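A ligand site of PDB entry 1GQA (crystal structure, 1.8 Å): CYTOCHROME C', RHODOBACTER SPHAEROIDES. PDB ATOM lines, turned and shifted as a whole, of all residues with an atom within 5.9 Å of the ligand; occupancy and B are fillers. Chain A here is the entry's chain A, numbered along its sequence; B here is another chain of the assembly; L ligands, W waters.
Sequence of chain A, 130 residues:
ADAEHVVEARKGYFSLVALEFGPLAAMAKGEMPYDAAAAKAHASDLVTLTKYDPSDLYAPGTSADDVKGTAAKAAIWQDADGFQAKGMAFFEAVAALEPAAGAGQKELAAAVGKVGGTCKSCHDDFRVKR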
ATOM      1  N   VAL A   7     -31.332  15.890  -7.176  1.00  0.00           N
ATOM      2  CA  VAL A   7     -30.276  16.683  -6.544  1.00  0.00           C
ATOM      3  C   VAL A   7     -30.287  16.486  -5.021  1.00  0.00           C
ATOM      4  O   VAL A   7     -29.239  16.271  -4.387  1.00  0.00           O
ATOM      5  CB  VAL A   7     -30.347  18.190  -6.927  1.00  0.00           C
ATOM      6  CG1 VAL A   7     -29.393  19.046  -5.982  1.00  0.00           C
ATOM      7  CG2 VAL A   7     -29.904  18.370  -8.355  1.00  0.00           C
ATOM      8  N   ARG A  10     -28.648  13.244  -4.272  1.00  0.00           N
ATOM      9  CA  ARG A  10     -27.222  13.216  -4.556  1.00  0.00           C
ATOM     10  C   ARG A  10     -26.449  13.872  -3.412  1.00  0.00           C
ATOM     11  O   ARG A  10     -25.443  13.362  -2.945  1.00  0.00           O
ATOM     12  CB  ARG A  10     -26.952  13.982  -5.842  1.00  0.00           C
ATOM     13  CG  ARG A  10     -25.501  13.926  -6.283  1.00  0.00           C
ATOM     14  CD  ARG A  10     -25.320  14.244  -7.799  1.00  0.00           C
ATOM     15  NE  ARG A  10     -25.740  15.596  -8.165  1.00  0.00           N
ATOM     16  CZ  ARG A  10     -26.481  15.882  -9.245  1.00  0.00           C
ATOM     17  NH1 ARG A  10     -26.945  14.977 -10.053  1.00  0.00           N
ATOM     18  NH2 ARG A  10     -26.821  17.074  -9.519  1.00  0.00           N
ATOM     19  N   LYS A  11     -26.911  15.015  -2.974  1.00  0.00           N
ATOM     20  CA  LYS A  11     -26.309  15.704  -1.860  1.00  0.00           C
ATOM     21  C   LYS A  11     -26.456  14.903  -0.565  1.00  0.00           C
ATOM     22  O   LYS A  11     -25.540  14.861   0.285  1.00  0.00           O
ATOM     23  CB  LYS A  11     -26.947  17.084  -1.743  1.00  0.00           C
ATOM     24  CG  LYS A  11     -26.649  17.977  -3.016  1.00  0.00           C
ATOM     25  CD  LYS A  11     -26.891  19.479  -2.792  1.00  0.00           C
ATOM     26  CE  LYS A  11     -28.336  19.787  -2.515  1.00  0.00           C
ATOM     27  NZ  LYS A  11     -28.546  21.267  -2.247  1.00  0.00           N
ATOM     28  N   GLY A  12     -27.618  14.247  -0.422  1.00  0.00           N
ATOM     29  CA  GLY A  12     -27.845  13.413   0.757  1.00  0.00           C
ATOM     30  C   GLY A  12     -26.791  12.313   0.805  1.00  0.00           C
ATOM     31  O   GLY A  12     -26.265  11.998   1.890  1.00  0.00           O
ATOM     32  N   PHE A  14     -23.752  12.275  -0.438  1.00  0.00           N
ATOM     33  CA  PHE A  14     -22.461  12.761   0.043  1.00  0.00           C
ATOM     34  C   PHE A  14     -22.541  13.194   1.496  1.00  0.00           C
ATOM     35  O   PHE A  14     -21.561  13.088   2.176  1.00  0.00           O
ATOM     36  CB  PHE A  14     -21.812  13.836  -0.880  1.00  0.00           C
ATOM     37  CG  PHE A  14     -21.409  13.276  -2.197  1.00  0.00           C
ATOM     38  CD1 PHE A  14     -20.306  12.471  -2.257  1.00  0.00           C
ATOM     39  CD2 PHE A  14     -22.159  13.454  -3.349  1.00  0.00           C
ATOM     40  CE1 PHE A  14     -19.904  11.809  -3.446  1.00  0.00           C
ATOM     41  CE2 PHE A  14     -21.786  12.821  -4.549  1.00  0.00           C
ATOM     42  CZ  PHE A  14     -20.667  12.040  -4.632  1.00  0.00           C
ATOM     43  N   SER A  15     -23.713  13.665   1.958  1.00  0.00           N
ATOM     44  CA  SER A  15     -23.851  13.993   3.380  1.00  0.00           C
ATOM     45  C   SER A  15     -23.556  12.753   4.250  1.00  0.00           C
ATOM     46  O   SER A  15     -22.890  12.878   5.296  1.00  0.00           O
ATOM     47  CB  SER A  15     -25.238  14.519   3.708  1.00  0.00           C
ATOM     48  OG  SER A  15     -25.365  15.832   3.268  1.00  0.00           O
ATOM     49  N   VAL A  17     -21.694  10.032   3.356  1.00  0.00           N
ATOM     50  CA  VAL A  17     -20.282   9.777   3.194  1.00  0.00           C
ATOM     51  C   VAL A  17     -19.539  10.711   4.168  1.00  0.00           C
ATOM     52  O   VAL A  17     -18.733  10.265   4.942  1.00  0.00           O
ATOM     53  CB  VAL A  17     -19.857  10.082   1.782  1.00  0.00           C
ATOM     54  CG1 VAL A  17     -18.370  10.054   1.645  1.00  0.00           C
ATOM     55  CG2 VAL A  17     -20.516   9.143   0.847  1.00  0.00           C
ATOM     56  N   ALA A  18     -19.849  11.998   4.161  1.00  0.00           N
ATOM     57  CA  ALA A  18     -19.132  12.921   5.023  1.00  0.00           C
ATOM     58  C   ALA A  18     -19.375  12.563   6.513  1.00  0.00           C
ATOM     59  O   ALA A  18     -18.445  12.661   7.318  1.00  0.00           O
ATOM     60  CB  ALA A  18     -19.546  14.333   4.739  1.00  0.00           C
ATOM     61  N   PHE A  21     -17.160   9.476   7.346  1.00  0.00           N
ATOM     62  CA  PHE A  21     -15.732   9.729   7.176  1.00  0.00           C
ATOM     63  C   PHE A  21     -15.211  10.705   8.222  1.00  0.00           C
ATOM     64  O   PHE A  21     -14.038  10.679   8.555  1.00  0.00           O
ATOM     65  CB  PHE A  21     -15.477  10.333   5.796  1.00  0.00           C
ATOM     66  CG  PHE A  21     -14.022  10.653   5.502  1.00  0.00           C
ATOM     67  CD1 PHE A  21     -13.607  11.975   5.421  1.00  0.00           C
ATOM     68  CD2 PHE A  21     -13.156   9.667   5.206  1.00  0.00           C
ATOM     69  CE1 PHE A  21     -12.274  12.297   5.104  1.00  0.00           C
ATOM     70  CE2 PHE A  21     -11.801   9.949   4.884  1.00  0.00           C
ATOM     71  CZ  PHE A  21     -11.378  11.270   4.816  1.00  0.00           C
ATOM     72  N   LEU A  46     -19.152   3.030   5.717  1.00  0.00           N
ATOM     73  CA  LEU A  46     -18.597   3.603   4.488  1.00  0.00           C
ATOM     74  C   LEU A  46     -18.469   2.567   3.350  1.00  0.00           C
ATOM     75  O   LEU A  46     -18.744   2.853   2.186  1.00  0.00           O
ATOM     76  CB  LEU A  46     -17.228   4.149   4.846  1.00  0.00           C
ATOM     77  CG  LEU A  46     -16.682   5.369   4.174  1.00  0.00           C
ATOM     78  CD1 LEU A  46     -17.813   6.314   3.725  1.00  0.00           C
ATOM     79  CD2 LEU A  46     -15.657   6.037   5.118  1.00  0.00           C
ATOM     80  N   TYR A  58     -27.252  10.292 -10.928  1.00  0.00           N
ATOM     81  CA  TYR A  58     -26.671  11.064 -12.029  1.00  0.00           C
ATOM     82  C   TYR A  58     -27.557  11.145 -13.281  1.00  0.00           C
ATOM     83  O   TYR A  58     -27.072  11.016 -14.390  1.00  0.00           O
ATOM     84  CB  TYR A  58     -25.260  10.556 -12.327  1.00  0.00           C
ATOM     85  CG  TYR A  58     -24.325  10.748 -11.153  1.00  0.00           C
ATOM     86  CD1 TYR A  58     -24.036   9.689 -10.299  1.00  0.00           C
ATOM     87  CD2 TYR A  58     -23.819  12.010 -10.844  1.00  0.00           C
ATOM     88  CE1 TYR A  58     -23.205   9.864  -9.231  1.00  0.00           C
ATOM     89  CE2 TYR A  58     -22.996  12.201  -9.760  1.00  0.00           C
ATOM     90  CZ  TYR A  58     -22.699  11.130  -8.939  1.00  0.00           C
ATOM     91  OH  TYR A  58     -21.865  11.329  -7.852  1.00  0.00           O
ATOM     92  N   GLY A  69     -28.684  24.886  -6.883  1.00  0.00           N
ATOM     93  CA  GLY A  69     -28.648  24.081  -5.689  1.00  0.00           C
ATOM     94  C   GLY A  69     -27.807  22.841  -5.877  1.00  0.00           C
ATOM     95  O   GLY A  69     -27.802  22.020  -4.971  1.00  0.00           O
ATOM     96  N   THR A  70     -27.104  22.706  -7.007  1.00  0.00           N
ATOM     97  CA  THR A  70     -26.192  21.565  -7.163  1.00  0.00           C
ATOM     98  C   THR A  70     -24.799  22.061  -7.490  1.00  0.00           C
ATOM     99  O   THR A  70     -24.659  23.154  -8.002  1.00  0.00           O
ATOM    100  CB  THR A  70     -26.642  20.527  -8.163  1.00  0.00           C
ATOM    101  OG1 THR A  70     -25.652  19.497  -8.249  1.00  0.00           O
ATOM    102  CG2 THR A  70     -26.701  21.065  -9.643  1.00  0.00           C
ATOM    103  N   ALA A  71     -23.770  21.249  -7.207  1.00  0.00           N
ATOM    104  CA  ALA A  71     -22.395  21.614  -7.469  1.00  0.00           C
ATOM    105  C   ALA A  71     -21.749  20.544  -8.375  1.00  0.00           C
ATOM    106  O   ALA A  71     -20.548  20.557  -8.611  1.00  0.00           O
ATOM    107  CB  ALA A  71     -21.588  21.707  -6.137  1.00  0.00           C
ATOM    108  N   ALA A  72     -22.602  19.650  -8.900  1.00  0.00           N
ATOM    109  CA  ALA A  72     -22.160  18.654  -9.867  1.00  0.00           C
ATOM    110  C   ALA A  72     -21.901  19.268 -11.256  1.00  0.00           C
ATOM    111  O   ALA A  72     -22.821  19.774 -11.905  1.00  0.00           O
ATOM    112  CB  ALA A  72     -23.128  17.553  -9.939  1.00  0.00           C
ATOM    113  N   LYS A  73     -20.650  19.175 -11.729  1.00  0.00           N
ATOM    114  CA  LYS A  73     -20.228  19.722 -12.995  1.00  0.00           C
ATOM    115  C   LYS A  73     -20.708  18.929 -14.205  1.00  0.00           C
ATOM    116  O   LYS A  73     -20.821  17.685 -14.159  1.00  0.00           O
ATOM    117  CB  LYS A  73     -18.721  19.829 -13.046  1.00  0.00           C
ATOM    118  CG  LYS A  73     -18.164  21.130 -12.526  1.00  0.00           C
ATOM    119  CD  LYS A  73     -16.842  21.389 -13.245  1.00  0.00           C
ATOM    120  CE  LYS A  73     -15.722  21.599 -12.279  1.00  0.00           C
ATOM    121  NZ  LYS A  73     -14.458  22.191 -12.981  1.00  0.00           N
ATOM    122  N   ILE A  76     -19.153  15.678 -15.478  1.00  0.00           N
ATOM    123  CA  ILE A  76     -19.470  14.319 -15.042  1.00  0.00           C
ATOM    124  C   ILE A  76     -20.089  13.557 -16.226  1.00  0.00           C
ATOM    125  O   ILE A  76     -19.737  12.424 -16.517  1.00  0.00           O
ATOM    126  CB  ILE A  76     -20.485  14.363 -13.840  1.00  0.00           C
ATOM    127  CG1 ILE A  76     -19.774  14.842 -12.568  1.00  0.00           C
ATOM    128  CG2 ILE A  76     -21.143  13.017 -13.592  1.00  0.00           C
ATOM    129  CD1 ILE A  76     -20.743  15.308 -11.449  1.00  0.00           C
ATOM    130  N   PHE A  83     -15.029   9.858 -14.809  1.00  0.00           N
ATOM    131  CA  PHE A  83     -15.827   9.813 -13.589  1.00  0.00           C
ATOM    132  C   PHE A  83     -15.821   8.432 -12.940  1.00  0.00           C
ATOM    133  O   PHE A  83     -15.622   8.353 -11.735  1.00  0.00           O
ATOM    134  CB  PHE A  83     -17.265  10.292 -13.805  1.00  0.00           C
ATOM    135  CG  PHE A  83     -17.987  10.664 -12.520  1.00  0.00           C
ATOM    136  CD1 PHE A  83     -19.100   9.954 -12.095  1.00  0.00           C
ATOM    137  CD2 PHE A  83     -17.543  11.722 -11.767  1.00  0.00           C
ATOM    138  CE1 PHE A  83     -19.769  10.261 -10.898  1.00  0.00           C
ATOM    139  CE2 PHE A  83     -18.206  12.087 -10.589  1.00  0.00           C
ATOM    140  CZ  PHE A  83     -19.303  11.355 -10.127  1.00  0.00           C
ATOM    141  N   LYS A  86     -12.540   7.928 -11.074  1.00  0.00           N
ATOM    142  CA  LYS A  86     -12.403   8.569  -9.774  1.00  0.00           C
ATOM    143  C   LYS A  86     -13.270   7.834  -8.755  1.00  0.00           C
ATOM    144  O   LYS A  86     -12.856   7.654  -7.627  1.00  0.00           O
ATOM    145  CB  LYS A  86     -12.638  10.087  -9.797  1.00  0.00           C
ATOM    146  CG  LYS A  86     -11.791  10.856 -10.873  1.00  0.00           C
ATOM    147  CD  LYS A  86     -10.414  11.383 -10.388  1.00  0.00           C
ATOM    148  CE  LYS A  86      -9.873  12.374 -11.418  1.00  0.00           C
ATOM    149  NZ  LYS A  86      -8.939  13.367 -10.826  1.00  0.00           N
ATOM    150  N   GLY A  87     -14.453   7.362  -9.168  1.00  0.00           N
ATOM    151  CA  GLY A  87     -15.303   6.544  -8.327  1.00  0.00           C
ATOM    152  C   GLY A  87     -14.621   5.251  -7.889  1.00  0.00           C
ATOM    153  O   GLY A  87     -14.631   4.873  -6.711  1.00  0.00           O
ATOM    154  N   PHE A  90     -11.936   5.675  -5.274  1.00  0.00           N
ATOM    155  CA  PHE A  90     -12.530   5.942  -3.970  1.00  0.00           C
ATOM    156  C   PHE A  90     -12.924   4.618  -3.379  1.00  0.00           C
ATOM    157  O   PHE A  90     -12.521   4.297  -2.285  1.00  0.00           O
ATOM    158  CB  PHE A  90     -13.752   6.830  -4.151  1.00  0.00           C
ATOM    159  CG  PHE A  90     -14.637   6.935  -2.961  1.00  0.00           C
ATOM    160  CD1 PHE A  90     -14.149   7.415  -1.742  1.00  0.00           C
ATOM    161  CD2 PHE A  90     -15.999   6.642  -3.069  1.00  0.00           C
ATOM    162  CE1 PHE A  90     -14.988   7.561  -0.676  1.00  0.00           C
ATOM    163  CE2 PHE A  90     -16.841   6.777  -1.994  1.00  0.00           C
ATOM    164  CZ  PHE A  90     -16.342   7.251  -0.800  1.00  0.00           C
ATOM    165  N   VAL A  94     -11.455   2.937   0.217  1.00  0.00           N
ATOM    166  CA  VAL A  94     -12.387   2.634   1.274  1.00  0.00           C
ATOM    167  C   VAL A  94     -12.239   1.148   1.679  1.00  0.00           C
ATOM    168  O   VAL A  94     -12.193   0.835   2.867  1.00  0.00           O
ATOM    169  CB  VAL A  94     -13.809   3.024   0.873  1.00  0.00           C
ATOM    170  CG1 VAL A  94     -14.890   2.473   1.830  1.00  0.00           C
ATOM    171  CG2 VAL A  94     -13.900   4.535   0.765  1.00  0.00           C
ATOM    172  N   VAL A 115      -7.863   7.730   1.402  1.00  0.00           N
ATOM    173  CA  VAL A 115      -9.250   7.998   1.119  1.00  0.00           C
ATOM    174  C   VAL A 115      -9.409   9.474   0.854  1.00  0.00           C
ATOM    175  O   VAL A 115     -10.015   9.886  -0.172  1.00  0.00           O
ATOM    176  CB  VAL A 115     -10.154   7.537   2.283  1.00  0.00           C
ATOM    177  CG1 VAL A 115     -11.584   7.908   2.002  1.00  0.00           C
ATOM    178  CG2 VAL A 115     -10.012   6.022   2.518  1.00  0.00           C
ATOM    179  N   GLY A 116      -8.898  10.289   1.777  1.00  0.00           N
ATOM    180  CA  GLY A 116      -9.014  11.744   1.617  1.00  0.00           C
ATOM    181  C   GLY A 116      -8.550  12.275   0.270  1.00  0.00           C
ATOM    182  O   GLY A 116      -9.174  13.141  -0.337  1.00  0.00           O
ATOM    183  N   THR A 118      -8.664  10.647  -2.467  1.00  0.00           N
ATOM    184  CA  THR A 118      -9.697  10.329  -3.422  1.00  0.00           C
ATOM    185  C   THR A 118     -10.861  11.330  -3.383  1.00  0.00           C
ATOM    186  O   THR A 118     -11.378  11.663  -4.420  1.00  0.00           O
ATOM    187  CB  THR A 118     -10.133   8.852  -3.440  1.00  0.00           C
ATOM    188  OG1 THR A 118     -10.988   8.523  -2.326  1.00  0.00           O
ATOM    189  CG2 THR A 118      -8.897   7.904  -3.388  1.00  0.00           C
ATOM    190  N   CYS A 119     -11.254  11.782  -2.210  1.00  0.00           N
ATOM    191  CA  CYS A 119     -12.289  12.794  -2.107  1.00  0.00           C
ATOM    192  C   CYS A 119     -11.891  13.977  -2.971  1.00  0.00           C
ATOM    193  O   CYS A 119     -12.659  14.419  -3.847  1.00  0.00           O
ATOM    194  CB  CYS A 119     -12.433  13.303  -0.702  1.00  0.00           C
ATOM    195  SG  CYS A 119     -12.753  11.983   0.470  1.00  0.00           S
ATOM    196  N   LYS A 120     -10.696  14.483  -2.705  1.00  0.00           N
ATOM    197  CA  LYS A 120     -10.258  15.712  -3.332  1.00  0.00           C
ATOM    198  C   LYS A 120     -10.077  15.584  -4.840  1.00  0.00           C
ATOM    199  O   LYS A 120     -10.430  16.502  -5.593  1.00  0.00           O
ATOM    200  CB  LYS A 120      -8.908  16.143  -2.779  1.00  0.00           C
ATOM    201  CG  LYS A 120      -8.303  17.327  -3.638  1.00  0.00           C
ATOM    202  CD  LYS A 120      -8.305  18.622  -2.865  1.00  0.00           C
ATOM    203  CE  LYS A 120      -7.978  19.847  -3.787  1.00  0.00           C
ATOM    204  NZ  LYS A 120      -6.732  19.754  -4.620  1.00  0.00           N
ATOM    205  N   CYS A 122     -11.528  13.659  -6.862  1.00  0.00           N
ATOM    206  CA  CYS A 122     -12.835  13.766  -7.545  1.00  0.00           C
ATOM    207  C   CYS A 122     -13.360  15.208  -7.592  1.00  0.00           C
ATOM    208  O   CYS A 122     -13.734  15.671  -8.646  1.00  0.00           O
ATOM    209  CB  CYS A 122     -13.888  12.892  -6.941  1.00  0.00           C
ATOM    210  SG  CYS A 122     -15.374  12.773  -8.014  1.00  0.00           S
ATOM    211  N   HIS A 123     -13.378  15.885  -6.458  1.00  0.00           N
ATOM    212  CA  HIS A 123     -13.821  17.243  -6.367  1.00  0.00           C
ATOM    213  C   HIS A 123     -13.096  18.120  -7.390  1.00  0.00           C
ATOM    214  O   HIS A 123     -13.701  18.963  -8.038  1.00  0.00           O
ATOM    215  CB  HIS A 123     -13.698  17.728  -4.907  1.00  0.00           C
ATOM    216  CG  HIS A 123     -14.555  16.933  -3.965  1.00  0.00           C
ATOM    217  ND1 HIS A 123     -14.353  16.896  -2.609  1.00  0.00           N
ATOM    218  CD2 HIS A 123     -15.668  16.187  -4.197  1.00  0.00           C
ATOM    219  CE1 HIS A 123     -15.284  16.126  -2.048  1.00  0.00           C
ATOM    220  NE2 HIS A 123     -16.084  15.663  -2.990  1.00  0.00           N
ATOM    221  N   PHE A 126     -14.670  17.342 -10.881  1.00  0.00           N
ATOM    222  CA  PHE A 126     -16.089  17.234 -11.132  1.00  0.00           C
ATOM    223  C   PHE A 126     -17.036  18.023 -10.235  1.00  0.00           C
ATOM    224  O   PHE A 126     -18.270  17.947 -10.420  1.00  0.00           O
ATOM    225  CB  PHE A 126     -16.493  15.762 -11.152  1.00  0.00           C
ATOM    226  CG  PHE A 126     -15.828  14.981 -12.241  1.00  0.00           C
ATOM    227  CD1 PHE A 126     -14.752  14.137 -11.977  1.00  0.00           C
ATOM    228  CD2 PHE A 126     -16.289  15.068 -13.542  1.00  0.00           C
ATOM    229  CE1 PHE A 126     -14.120  13.399 -12.996  1.00  0.00           C
ATOM    230  CE2 PHE A 126     -15.675  14.323 -14.575  1.00  0.00           C
ATOM    231  CZ  PHE A 126     -14.574  13.501 -14.298  1.00  0.00           C
ATOM    232  N   ARG A 127     -16.493  18.755  -9.261  1.00  0.00           N
ATOM    233  CA  ARG A 127     -17.318  19.550  -8.398  1.00  0.00           C
ATOM    234  C   ARG A 127     -16.985  21.028  -8.578  1.00  0.00           C
ATOM    235  O   ARG A 127     -15.831  21.383  -8.548  1.00  0.00           O
ATOM    236  CB  ARG A 127     -17.158  19.154  -6.917  1.00  0.00           C
ATOM    237  CG  ARG A 127     -18.066  19.922  -6.005  1.00  0.00           C
ATOM    238  CD  ARG A 127     -18.029  19.471  -4.557  1.00  0.00           C
ATOM    239  NE  ARG A 127     -16.819  19.938  -3.917  1.00  0.00           N
ATOM    240  CZ  ARG A 127     -16.523  19.709  -2.646  1.00  0.00           C
ATOM    241  NH1 ARG A 127     -15.398  20.212  -2.133  1.00  0.00           N
ATOM    242  NH2 ARG A 127     -17.352  18.976  -1.889  1.00  0.00           N
ATOM    243  N   GLU B   8     -28.989  16.831   8.221  1.00  0.00           N
ATOM    244  CA  GLU B   8     -28.818  16.690   6.751  1.00  0.00           C
ATOM    245  C   GLU B   8     -28.561  15.245   6.274  1.00  0.00           C
ATOM    246  O   GLU B   8     -29.025  14.865   5.191  1.00  0.00           O
ATOM    247  CB  GLU B   8     -27.695  17.617   6.213  1.00  0.00           C
ATOM    248  CG  GLU B   8     -27.650  17.689   4.681  1.00  0.00           C
ATOM    249  CD  GLU B   8     -26.805  18.821   4.126  1.00  0.00           C
ATOM    250  OE1 GLU B   8     -27.027  19.246   2.943  1.00  0.00           O
ATOM    251  OE2 GLU B   8     -25.901  19.275   4.831  1.00  0.00           O
HETATM  252 FE1  LIG L   1     -17.675  14.585  -2.679  1.00  0.00          FE
HETATM  253  C1  LIG L   1     -20.216  16.865  -2.876  1.00  0.00           C
HETATM  254  C2  LIG L   1     -17.605  14.971   0.737  1.00  0.00           C
HETATM  255  C3  LIG L   1     -15.686  11.801  -2.277  1.00  0.00           C
HETATM  256  C4  LIG L   1     -18.068  13.888  -6.010  1.00  0.00           C
HETATM  257  N1  LIG L   1     -18.784  15.770  -1.230  1.00  0.00           N
HETATM  258  C5  LIG L   1     -19.719  16.597  -1.570  1.00  0.00           C
HETATM  259  C6  LIG L   1     -20.063  17.295  -0.428  1.00  0.00           C
HETATM  260  C7  LIG L   1     -19.337  16.698   0.643  1.00  0.00           C
HETATM  261  C8  LIG L   1     -18.547  15.737   0.044  1.00  0.00           C
HETATM  262  C9  LIG L   1     -19.385  17.075   2.100  1.00  0.00           C
HETATM  263  C10 LIG L   1     -21.219  18.291  -0.336  1.00  0.00           C
HETATM  264  C11 LIG L   1     -22.556  17.693  -0.070  1.00  0.00           C
HETATM  265  C12 LIG L   1     -23.665  18.749   0.154  1.00  0.00           C
HETATM  266  O1  LIG L   1     -24.338  18.778   1.197  1.00  0.00           O
HETATM  267  O2  LIG L   1     -24.024  19.502  -0.758  1.00  0.00           O
HETATM  268  N2  LIG L   1     -16.773  13.411  -1.099  1.00  0.00           N
HETATM  269  C13 LIG L   1     -16.824  13.889   0.284  1.00  0.00           C
HETATM  270  C14 LIG L   1     -15.922  13.126   1.054  1.00  0.00           C
HETATM  271  C15 LIG L   1     -15.372  12.195   0.181  1.00  0.00           C
HETATM  272  C16 LIG L   1     -15.947  12.428  -1.072  1.00  0.00           C
HETATM  273  C17 LIG L   1     -15.698  13.338   2.539  1.00  0.00           C
HETATM  274  C18 LIG L   1     -14.456  11.172   0.466  1.00  0.00           C
HETATM  275  C19 LIG L   1     -14.550  10.314   1.615  1.00  0.00           C
HETATM  276  N3  LIG L   1     -16.994  13.054  -3.915  1.00  0.00           N
HETATM  277  C20 LIG L   1     -16.136  12.074  -3.603  1.00  0.00           C
HETATM  278  C21 LIG L   1     -15.881  11.282  -4.722  1.00  0.00           C
HETATM  279  C22 LIG L   1     -16.516  11.918  -5.801  1.00  0.00           C
HETATM  280  C23 LIG L   1     -17.245  12.990  -5.307  1.00  0.00           C
HETATM  281  C24 LIG L   1     -14.908  10.067  -4.794  1.00  0.00           C
HETATM  282  C25 LIG L   1     -16.491  11.526  -7.162  1.00  0.00           C
HETATM  283  C26 LIG L   1     -16.646  10.199  -7.687  1.00  0.00           C
HETATM  284  N4  LIG L   1     -19.078  15.308  -4.330  1.00  0.00           N
HETATM  285  C27 LIG L   1     -18.913  14.857  -5.502  1.00  0.00           C
HETATM  286  C28 LIG L   1     -19.787  15.648  -6.251  1.00  0.00           C
HETATM  287  C29 LIG L   1     -20.398  16.518  -5.350  1.00  0.00           C
HETATM  288  C30 LIG L   1     -19.895  16.196  -4.083  1.00  0.00           C
HETATM  289  C31 LIG L   1     -20.013  15.586  -7.743  1.00  0.00           C
HETATM  290  C32 LIG L   1     -21.476  17.596  -5.658  1.00  0.00           C
HETATM  291  C33 LIG L   1     -22.900  17.084  -5.373  1.00  0.00           C
HETATM  292  C34 LIG L   1     -24.022  18.062  -5.746  1.00  0.00           C
HETATM  293  O3  LIG L   1     -23.848  19.242  -5.494  1.00  0.00           O
HETATM  294  O4  LIG L   1     -24.896  17.692  -6.498  1.00  0.00           O
HETATM  295  O   HOH W   1     -16.922  16.361   4.137  1.00  0.00           O
HETATM  296  O   HOH W   2     -22.685  20.108  -3.115  1.00  0.00           O
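The side-chain hydroxyl (OG1) of Thr 70 lies within hydrogen-bond range of an oxygen (O4) of the ligand (2.6 Å).
The guanidinium group (NE) of Arg 10 lies within salt-bridge range of an oxygen (O4) of the ligand (2.8 Å).
SG of Cys 122 is covalently linked to C25 of the ligand, 1.9 Å away.
N of Ala 71 lies within hydrogen-bond range of O3 of the ligand, at 2.6 Å.
The side-chain sulfur (SG) of Cys 119 is bonded to a carbon (C18) of the ligand (1.9 Å).
A ring nitrogen (NE2) of His 123 is bound to an iron atom (FE1) of the ligand (1.9 Å).
OG1 of Thr 70 lies within hydrogen-bond range of NH2 of Arg 10 (3.0 Å).
O of Cys 119 sits close to ND1 of His 123, 3.2 Å away.
The side-chain amino group (NZ) of Lys 11 lies within hydrogen-bond range of the backbone carbonyl oxygen (O) of Gly 69 (2.9 Å).
OG1 of Thr 118 sits at hydrogen-bond distance from O of Val 115 (2.7 Å).
OG1 of Thr 70 is in hydrogen-bond range of N of Ala 72, at 3.1 Å.
O of Phe 126 sits at hydrogen-bond distance from N of Lys 73 (3.0 Å).
The backbone carbonyl oxygen (O) of Lys 11 sits at hydrogen-bond distance from the side-chain hydroxyl (OG) of Ser 15 (3.1 Å).
An oxygen (O1) of the ligand sits close to the side-chain carboxylate (OE1) of Glu 8 of chain B (3.2 Å).
Lys 11 touches the ligand (CD to O2, 3.5 Å).
CE1 of Phe 14 touches N3 of the ligand, at 3.2 Å.
Ser 15 touches the ligand (OG to O1, 3.7 Å).
Val 17 touches the ligand (CG1 to C19, 3.8 Å).
Ala 18 touches the ligand (CB to C9, 3.8 Å).
Phe 21 touches the ligand.
N of Ala 72 touches O3 of the ligand (3.6 Å).
Ile 76 touches the ligand (CD1 to C31, 3.8 Å).
Phe 83 touches the ligand.
Gly 87 touches the ligand.
CB of Phe 90 touches C24 of the ligand (3.5 Å).
Val 115 touches the ligand.
Thr 118 touches the ligand (O to C24, 3.9 Å).
Phe 126 touches the ligand (O to C31, 3.97 Å).
Arg 127 touches the ligand (NH2 to C5, 3.4 Å).
22 residues have an atom within 4 Å of the ligand: Arg 10, Lys 11, Phe 14, Ser 15, Val 17, Ala 18, Phe 21, Thr 70, Ala 71, Ala 72, Ile 76, Phe 83, Gly 87, Phe 90, Val 115, Thr 118, Cys 119, Cys 122, His 123, Phe 126, Arg 127 and Glu 8 of chain B.
The nearest printed residue that does not touch the ligand is Lys 86 (4.2 Å).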
